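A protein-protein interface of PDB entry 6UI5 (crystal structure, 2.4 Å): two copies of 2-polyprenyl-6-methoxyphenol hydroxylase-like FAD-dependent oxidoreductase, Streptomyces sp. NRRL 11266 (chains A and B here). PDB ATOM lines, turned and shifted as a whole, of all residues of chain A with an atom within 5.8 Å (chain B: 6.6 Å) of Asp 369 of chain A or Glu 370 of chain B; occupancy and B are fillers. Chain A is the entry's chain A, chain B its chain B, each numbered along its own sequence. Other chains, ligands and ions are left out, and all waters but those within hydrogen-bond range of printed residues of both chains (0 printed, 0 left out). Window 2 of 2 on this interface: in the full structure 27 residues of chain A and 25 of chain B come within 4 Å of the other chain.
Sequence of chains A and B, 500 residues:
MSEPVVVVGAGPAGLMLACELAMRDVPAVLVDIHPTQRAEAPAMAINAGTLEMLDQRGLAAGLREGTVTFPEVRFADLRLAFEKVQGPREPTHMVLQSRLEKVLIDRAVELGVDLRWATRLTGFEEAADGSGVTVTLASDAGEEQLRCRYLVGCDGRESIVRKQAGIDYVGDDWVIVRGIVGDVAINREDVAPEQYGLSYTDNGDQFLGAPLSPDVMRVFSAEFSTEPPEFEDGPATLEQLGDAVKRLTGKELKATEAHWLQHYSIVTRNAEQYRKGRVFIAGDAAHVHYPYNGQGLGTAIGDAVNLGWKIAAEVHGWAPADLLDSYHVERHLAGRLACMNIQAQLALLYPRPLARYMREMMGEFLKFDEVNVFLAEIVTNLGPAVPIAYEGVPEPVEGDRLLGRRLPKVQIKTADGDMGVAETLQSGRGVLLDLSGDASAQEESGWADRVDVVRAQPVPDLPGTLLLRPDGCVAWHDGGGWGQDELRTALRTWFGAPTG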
ATOM      1  N   LYS A  84      13.544  -4.167 -18.750  1.00  0.00           N
ATOM      2  CA  LYS A  84      14.749  -3.799 -18.019  1.00  0.00           C
ATOM      3  C   LYS A  84      15.047  -2.304 -18.095  1.00  0.00           C
ATOM      4  O   LYS A  84      15.976  -1.831 -17.441  1.00  0.00           O
ATOM      5  CB  LYS A  84      15.950  -4.609 -18.543  1.00  0.00           C
ATOM      6  CG  LYS A  84      15.744  -6.133 -18.545  1.00  0.00           C
ATOM      7  CD  LYS A  84      16.578  -6.857 -17.485  1.00  0.00           C
ATOM      8  CE  LYS A  84      16.057  -6.635 -16.055  1.00  0.00           C
ATOM      9  NZ  LYS A  84      17.026  -7.124 -15.010  1.00  0.00           N
ATOM     10  N   PHE A 365      24.843 -11.251 -27.493  1.00  0.00           N
ATOM     11  CA  PHE A 365      24.882  -9.961 -26.807  1.00  0.00           C
ATOM     12  C   PHE A 365      23.573  -9.670 -26.081  1.00  0.00           C
ATOM     13  O   PHE A 365      23.578  -9.105 -24.979  1.00  0.00           O
ATOM     14  CB  PHE A 365      25.194  -8.841 -27.796  1.00  0.00           C
ATOM     15  CG  PHE A 365      26.611  -8.833 -28.308  1.00  0.00           C
ATOM     16  CD1 PHE A 365      27.551  -9.724 -27.826  1.00  0.00           C
ATOM     17  CD2 PHE A 365      27.014  -7.880 -29.243  1.00  0.00           C
ATOM     18  CE1 PHE A 365      28.854  -9.693 -28.289  1.00  0.00           C
ATOM     19  CE2 PHE A 365      28.314  -7.850 -29.721  1.00  0.00           C
ATOM     20  CZ  PHE A 365      29.238  -8.760 -29.242  1.00  0.00           C
ATOM     21  N   LYS A 367      21.893 -11.587 -24.480  1.00  0.00           N
ATOM     22  CA  LYS A 367      21.799 -12.217 -23.171  1.00  0.00           C
ATOM     23  C   LYS A 367      22.214 -11.276 -22.057  1.00  0.00           C
ATOM     24  O   LYS A 367      21.990 -11.602 -20.892  1.00  0.00           O
ATOM     25  CB  LYS A 367      22.650 -13.491 -23.119  1.00  0.00           C
ATOM     26  CG  LYS A 367      22.048 -14.655 -23.905  1.00  0.00           C
ATOM     27  CD  LYS A 367      23.075 -15.728 -24.236  1.00  0.00           C
ATOM     28  CE  LYS A 367      22.445 -16.849 -25.054  1.00  0.00           C
ATOM     29  NZ  LYS A 367      23.320 -18.048 -25.169  1.00  0.00           N
ATOM     30  N   PHE A 368      22.786 -10.118 -22.388  1.00  0.00           N
ATOM     31  CA  PHE A 368      23.303  -9.157 -21.420  1.00  0.00           C
ATOM     32  C   PHE A 368      22.312  -8.027 -21.164  1.00  0.00           C
ATOM     33  O   PHE A 368      21.691  -7.502 -22.092  1.00  0.00           O
ATOM     34  CB  PHE A 368      24.619  -8.547 -21.904  1.00  0.00           C
ATOM     35  CG  PHE A 368      25.653  -9.555 -22.300  1.00  0.00           C
ATOM     36  CD1 PHE A 368      25.842 -10.718 -21.550  1.00  0.00           C
ATOM     37  CD2 PHE A 368      26.443  -9.339 -23.428  1.00  0.00           C
ATOM     38  CE1 PHE A 368      26.808 -11.657 -21.920  1.00  0.00           C
ATOM     39  CE2 PHE A 368      27.409 -10.265 -23.813  1.00  0.00           C
ATOM     40  CZ  PHE A 368      27.593 -11.431 -23.060  1.00  0.00           C
ATOM     41  N   ASP A 369      22.211  -7.618 -19.898  1.00  0.00           N
ATOM     42  CA  ASP A 369      21.257  -6.580 -19.527  1.00  0.00           C
ATOM     43  C   ASP A 369      21.655  -5.216 -20.092  1.00  0.00           C
ATOM     44  O   ASP A 369      20.802  -4.474 -20.595  1.00  0.00           O
ATOM     45  CB  ASP A 369      21.128  -6.520 -18.003  1.00  0.00           C
ATOM     46  CG  ASP A 369      20.559  -7.801 -17.408  1.00  0.00           C
ATOM     47  OD1 ASP A 369      20.386  -8.796 -18.157  1.00  0.00           O
ATOM     48  OD2 ASP A 369      20.291  -7.806 -16.185  1.00  0.00           O
ATOM     49  N   GLU A 370      22.937  -4.850 -19.999  1.00  0.00           N
ATOM     50  CA  GLU A 370      23.340  -3.527 -20.466  1.00  0.00           C
ATOM     51  C   GLU A 370      23.107  -3.365 -21.956  1.00  0.00           C
ATOM     52  O   GLU A 370      22.843  -2.252 -22.415  1.00  0.00           O
ATOM     53  CB  GLU A 370      24.811  -3.244 -20.143  1.00  0.00           C
ATOM     54  CG  GLU A 370      25.028  -2.662 -18.728  1.00  0.00           C
ATOM     55  CD  GLU A 370      26.484  -2.305 -18.415  1.00  0.00           C
ATOM     56  OE1 GLU A 370      26.727  -1.156 -17.988  1.00  0.00           O
ATOM     57  OE2 GLU A 370      27.377  -3.167 -18.580  1.00  0.00           O
ATOM     58  N   VAL A 371      23.222  -4.447 -22.735  1.00  0.00           N
ATOM     59  CA  VAL A 371      22.982  -4.302 -24.163  1.00  0.00           C
ATOM     60  C   VAL A 371      21.497  -4.104 -24.419  1.00  0.00           C
ATOM     61  O   VAL A 371      21.099  -3.169 -25.134  1.00  0.00           O
ATOM     62  CB  VAL A 371      23.545  -5.498 -24.947  1.00  0.00           C
ATOM     63  CG1 VAL A 371      23.102  -5.407 -26.415  1.00  0.00           C
ATOM     64  CG2 VAL A 371      25.090  -5.543 -24.834  1.00  0.00           C
ATOM     65  N   ASN A 372      20.652  -4.943 -23.796  1.00  0.00           N
ATOM     66  CA  ASN A 372      19.205  -4.822 -23.968  1.00  0.00           C
ATOM     67  C   ASN A 372      18.734  -3.424 -23.611  1.00  0.00           C
ATOM     68  O   ASN A 372      17.979  -2.795 -24.368  1.00  0.00           O
ATOM     69  CB  ASN A 372      18.473  -5.854 -23.117  1.00  0.00           C
ATOM     70  CG  ASN A 372      18.295  -7.175 -23.836  1.00  0.00           C
ATOM     71  OD1 ASN A 372      17.301  -7.402 -24.545  1.00  0.00           O
ATOM     72  ND2 ASN A 372      19.270  -8.057 -23.666  1.00  0.00           N
ATOM     73  N   VAL A 373      19.202  -2.901 -22.480  1.00  0.00           N
ATOM     74  CA  VAL A 373      18.720  -1.603 -22.038  1.00  0.00           C
ATOM     75  C   VAL A 373      19.216  -0.511 -22.972  1.00  0.00           C
ATOM     76  O   VAL A 373      18.451   0.368 -23.389  1.00  0.00           O
ATOM     77  CB  VAL A 373      19.136  -1.364 -20.577  1.00  0.00           C
ATOM     78  CG1 VAL A 373      18.893   0.090 -20.167  1.00  0.00           C
ATOM     79  CG2 VAL A 373      18.365  -2.344 -19.697  1.00  0.00           C
ATOM     80  N   PHE A 374      20.484  -0.582 -23.365  1.00  0.00           N
ATOM     81  CA  PHE A 374      21.038   0.451 -24.229  1.00  0.00           C
ATOM     82  C   PHE A 374      20.285   0.530 -25.552  1.00  0.00           C
ATOM     83  O   PHE A 374      19.832   1.612 -25.948  1.00  0.00           O
ATOM     84  CB  PHE A 374      22.515   0.192 -24.479  1.00  0.00           C
ATOM     85  CG  PHE A 374      23.091   1.015 -25.599  1.00  0.00           C
ATOM     86  CD1 PHE A 374      23.409   2.347 -25.401  1.00  0.00           C
ATOM     87  CD2 PHE A 374      23.366   0.440 -26.829  1.00  0.00           C
ATOM     88  CE1 PHE A 374      23.955   3.098 -26.410  1.00  0.00           C
ATOM     89  CE2 PHE A 374      23.925   1.183 -27.844  1.00  0.00           C
ATOM     90  CZ  PHE A 374      24.222   2.519 -27.633  1.00  0.00           C
ATOM     91  N   PHE B 365      29.002  -1.334 -27.838  1.00  0.00           N
ATOM     92  CA  PHE B 365      28.944  -2.535 -27.004  1.00  0.00           C
ATOM     93  C   PHE B 365      30.178  -2.652 -26.111  1.00  0.00           C
ATOM     94  O   PHE B 365      30.061  -2.938 -24.910  1.00  0.00           O
ATOM     95  CB  PHE B 365      28.776  -3.775 -27.873  1.00  0.00           C
ATOM     96  CG  PHE B 365      27.438  -3.843 -28.570  1.00  0.00           C
ATOM     97  CD1 PHE B 365      26.327  -3.230 -28.015  1.00  0.00           C
ATOM     98  CD2 PHE B 365      27.297  -4.491 -29.774  1.00  0.00           C
ATOM     99  CE1 PHE B 365      25.091  -3.278 -28.642  1.00  0.00           C
ATOM    100  CE2 PHE B 365      26.055  -4.531 -30.422  1.00  0.00           C
ATOM    101  CZ  PHE B 365      24.949  -3.931 -29.848  1.00  0.00           C
ATOM    102  N   PHE B 368      30.399  -1.850 -22.546  1.00  0.00           N
ATOM    103  CA  PHE B 368      29.765  -2.698 -21.543  1.00  0.00           C
ATOM    104  C   PHE B 368      30.747  -3.770 -21.080  1.00  0.00           C
ATOM    105  O   PHE B 368      31.498  -4.335 -21.883  1.00  0.00           O
ATOM    106  CB  PHE B 368      28.494  -3.339 -22.106  1.00  0.00           C
ATOM    107  CG  PHE B 368      27.483  -2.332 -22.583  1.00  0.00           C
ATOM    108  CD1 PHE B 368      27.425  -1.077 -22.014  1.00  0.00           C
ATOM    109  CD2 PHE B 368      26.606  -2.633 -23.594  1.00  0.00           C
ATOM    110  CE1 PHE B 368      26.519  -0.150 -22.441  1.00  0.00           C
ATOM    111  CE2 PHE B 368      25.700  -1.699 -24.031  1.00  0.00           C
ATOM    112  CZ  PHE B 368      25.660  -0.454 -23.450  1.00  0.00           C
ATOM    113  N   ASP B 369      30.741  -4.039 -19.773  1.00  0.00           N
ATOM    114  CA  ASP B 369      31.726  -4.951 -19.210  1.00  0.00           C
ATOM    115  C   ASP B 369      31.438  -6.405 -19.565  1.00  0.00           C
ATOM    116  O   ASP B 369      32.384  -7.182 -19.762  1.00  0.00           O
ATOM    117  CB  ASP B 369      31.794  -4.779 -17.697  1.00  0.00           C
ATOM    118  CG  ASP B 369      32.608  -3.572 -17.298  1.00  0.00           C
ATOM    119  OD1 ASP B 369      33.347  -3.047 -18.170  1.00  0.00           O
ATOM    120  OD2 ASP B 369      32.503  -3.159 -16.120  1.00  0.00           O
ATOM    121  N   GLU B 370      30.159  -6.802 -19.637  1.00  0.00           N
ATOM    122  CA  GLU B 370      29.858  -8.191 -19.972  1.00  0.00           C
ATOM    123  C   GLU B 370      30.280  -8.536 -21.391  1.00  0.00           C
ATOM    124  O   GLU B 370      30.690  -9.670 -21.652  1.00  0.00           O
ATOM    125  CB  GLU B 370      28.375  -8.492 -19.807  1.00  0.00           C
ATOM    126  CG  GLU B 370      27.885  -8.370 -18.393  1.00  0.00           C
ATOM    127  CD  GLU B 370      26.397  -8.624 -18.299  1.00  0.00           C
ATOM    128  OE1 GLU B 370      25.969  -9.753 -18.622  1.00  0.00           O
ATOM    129  OE2 GLU B 370      25.652  -7.691 -17.928  1.00  0.00           O
ATOM    130  N   VAL B 371      30.189  -7.595 -22.324  1.00  0.00           N
ATOM    131  CA  VAL B 371      30.576  -7.985 -23.669  1.00  0.00           C
ATOM    132  C   VAL B 371      32.091  -7.990 -23.780  1.00  0.00           C
ATOM    133  O   VAL B 371      32.661  -8.842 -24.475  1.00  0.00           O
ATOM    134  CB  VAL B 371      29.885  -7.096 -24.720  1.00  0.00           C
ATOM    135  CG1 VAL B 371      28.519  -6.689 -24.210  1.00  0.00           C
ATOM    136  CG2 VAL B 371      30.705  -5.888 -25.075  1.00  0.00           C
ATOM    137  N   ASN B 372      32.779  -7.100 -23.065  1.00  0.00           N
ATOM    138  CA  ASN B 372      34.231  -7.203 -23.051  1.00  0.00           C
ATOM    139  C   ASN B 372      34.669  -8.540 -22.479  1.00  0.00           C
ATOM    140  O   ASN B 372      35.553  -9.196 -23.034  1.00  0.00           O
ATOM    141  CB  ASN B 372      34.849  -6.068 -22.258  1.00  0.00           C
ATOM    142  CG  ASN B 372      35.109  -4.865 -23.106  1.00  0.00           C
ATOM    143  OD1 ASN B 372      36.157  -4.754 -23.764  1.00  0.00           O
ATOM    144  ND2 ASN B 372      34.152  -3.941 -23.105  1.00  0.00           N
ATOM    145  N   VAL B 373      34.021  -8.991 -21.403  1.00  0.00           N
ATOM    146  CA  VAL B 373      34.450 -10.228 -20.757  1.00  0.00           C
ATOM    147  C   VAL B 373      34.052 -11.436 -21.598  1.00  0.00           C
ATOM    148  O   VAL B 373      34.856 -12.351 -21.817  1.00  0.00           O
ATOM    149  CB  VAL B 373      33.897 -10.307 -19.322  1.00  0.00           C
ATOM    150  CG1 VAL B 373      33.962 -11.729 -18.798  1.00  0.00           C
ATOM    151  CG2 VAL B 373      34.705  -9.360 -18.385  1.00  0.00           C
ATOM    152  N   PHE B 374      32.817 -11.441 -22.104  1.00  0.00           N
ATOM    153  CA  PHE B 374      32.378 -12.517 -22.993  1.00  0.00           C
ATOM    154  C   PHE B 374      33.296 -12.661 -24.200  1.00  0.00           C
ATOM    155  O   PHE B 374      33.732 -13.773 -24.527  1.00  0.00           O
ATOM    156  CB  PHE B 374      30.942 -12.291 -23.463  1.00  0.00           C
ATOM    157  CG  PHE B 374      30.479 -13.318 -24.460  1.00  0.00           C
ATOM    158  CD1 PHE B 374      30.203 -14.616 -24.059  1.00  0.00           C
ATOM    159  CD2 PHE B 374      30.341 -12.995 -25.807  1.00  0.00           C
ATOM    160  CE1 PHE B 374      29.782 -15.572 -24.980  1.00  0.00           C
ATOM    161  CE2 PHE B 374      29.922 -13.942 -26.719  1.00  0.00           C
ATOM    162  CZ  PHE B 374      29.644 -15.233 -26.305  1.00  0.00           C
ATOM    163  N   LEU B 375      33.601 -11.551 -24.881  1.00  0.00           N
ATOM    164  CA  LEU B 375      34.442 -11.666 -26.069  1.00  0.00           C
ATOM    165  C   LEU B 375      35.850 -12.116 -25.696  1.00  0.00           C
ATOM    166  O   LEU B 375      36.468 -12.921 -26.414  1.00  0.00           O
ATOM    167  CB  LEU B 375      34.463 -10.340 -26.836  1.00  0.00           C
ATOM    168  CG  LEU B 375      33.149 -10.043 -27.571  1.00  0.00           C
ATOM    169  CD1 LEU B 375      33.253  -8.754 -28.354  1.00  0.00           C
ATOM    170  CD2 LEU B 375      32.836 -11.174 -28.501  1.00  0.00           C
ATOM    171  N   ARG B 401      31.249 -18.067 -11.973  1.00  0.00           N
ATOM    172  CA  ARG B 401      31.986 -18.247 -13.216  1.00  0.00           C
ATOM    173  C   ARG B 401      33.186 -19.169 -13.049  1.00  0.00           C
ATOM    174  O   ARG B 401      34.222 -18.971 -13.686  1.00  0.00           O
ATOM    175  CB  ARG B 401      32.424 -16.907 -13.808  1.00  0.00           C
ATOM    176  CG  ARG B 401      31.902 -16.768 -15.229  1.00  0.00           C
ATOM    177  CD  ARG B 401      32.654 -15.755 -16.087  1.00  0.00           C
ATOM    178  NE  ARG B 401      31.957 -14.478 -16.109  1.00  0.00           N
ATOM    179  CZ  ARG B 401      30.848 -14.265 -16.806  1.00  0.00           C
ATOM    180  NH1 ARG B 401      30.329 -15.253 -17.531  1.00  0.00           N
ATOM    181  NH2 ARG B 401      30.255 -13.073 -16.773  1.00  0.00           N
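Of chain B, only Glu 370 (3.97 Å) comes within 4 Å of Asp 369 of chain A. Of the printed residues of chain A, Glu 370 of chain B touches Phe 368 (3.1 Å) and Asp 369 (3.97 Å). Of the printed residues of chain A, Asp 369 of chain B touches Glu 370. Of the printed residues of chain B, Glu 370 of chain A touches Phe 368 and Asp 369. Printed residues of chain A within 4 Å of Phe 365 of chain B: Phe 365 and Val 371. Of the printed residues of chain B, Phe 368 of chain A touches Glu 370, Val 371 and Phe 374. Of the printed residues of chain B, Phe 374 of chain A touches Phe 368 (3.4 Å). Asn 372 of chain B touches none of the printed residues of chain A. Val 373 of chain A touches none of the printed residues of chain B. The nearest printed residue of chain B that does not touch Asp 369 of chain A is Phe 368 of chain B (6.6 Å).
The backbone carbonyl oxygen (O) of Phe 368 of chain B is in hydrogen-bond range of the side-chain amide nitrogen (ND2) of Asn 372 of chain B, 2.9 Å away. ND2 of Asn 372 of chain A sits at hydrogen-bond distance from O of Phe 368 of chain A (2.9 Å). The side-chain amino group (NZ) of Lys 84 of chain A is in salt-bridge range of the side-chain carboxylate (OD2) of Asp 369 of chain A, 3.5 Å away.
Phe 365 of chain A touches Phe 365 of chain B. Phe 368 of chain A touches Glu 370 of chain B. CD2 of Phe 368 of chain A touches CG1 of Val 371 of chain B (3.5 Å). Phe 374 of chain B touches Phe 368 of chain A (CB to CZ, 3.5 Å). Glu 370 of chain B touches Asp 369 of chain A (OE2 to N, 3.97 Å). Phe 368 of chain B touches Glu 370 of chain A. Glu 370 of chain A touches Asp 369 of chain B. Phe 365 of chain B touches Val 371 of chain A (CE1 to CG1, 3.7 Å). CG2 of Val 371 of chain A touches CG1 of Val 371 of chain B, at 3.7 Å. Phe 368 of chain B touches Phe 374 of chain A (CZ to CB, 3.4 Å).
Phe 368 of chain A touches Val 371 of chain B, and with the chains exchanged Val 371 of chain A touches Phe 368 of chain B. Phe 368 of chain A touches Phe 374 of chain B, and with the chains exchanged Phe 374 of chain A touches Phe 368 of chain B. Asp 369 of chain A touches Glu 370 of chain B, and with the chains exchanged Glu 370 of chain A touches Asp 369 of chain B. Val 371 of chain A touches its own counterpart, Val 371 of chain B. 8 positions are printed for both chains. Of the 11 pairs that touch across the chains among the printed residues, 10 have their exchanged pair printed and touching as well.
Printed residues of chain B that touch a printed residue of chain A: Phe 365, Phe 368, Asp 369, Glu 370, Val 371 and Phe 374. Hydrophobic or aromatic side chains of chain B within 4 Å of the printed part of chain A: Phe 365, Phe 368, Val 371 and Phe 374. Among the printed residues, 11 pairs touch across the chains. Among the printed residues, no Asp or Glu carboxylate lies within 4 Å of a Lys or Arg side-chain nitrogen of the other chain.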
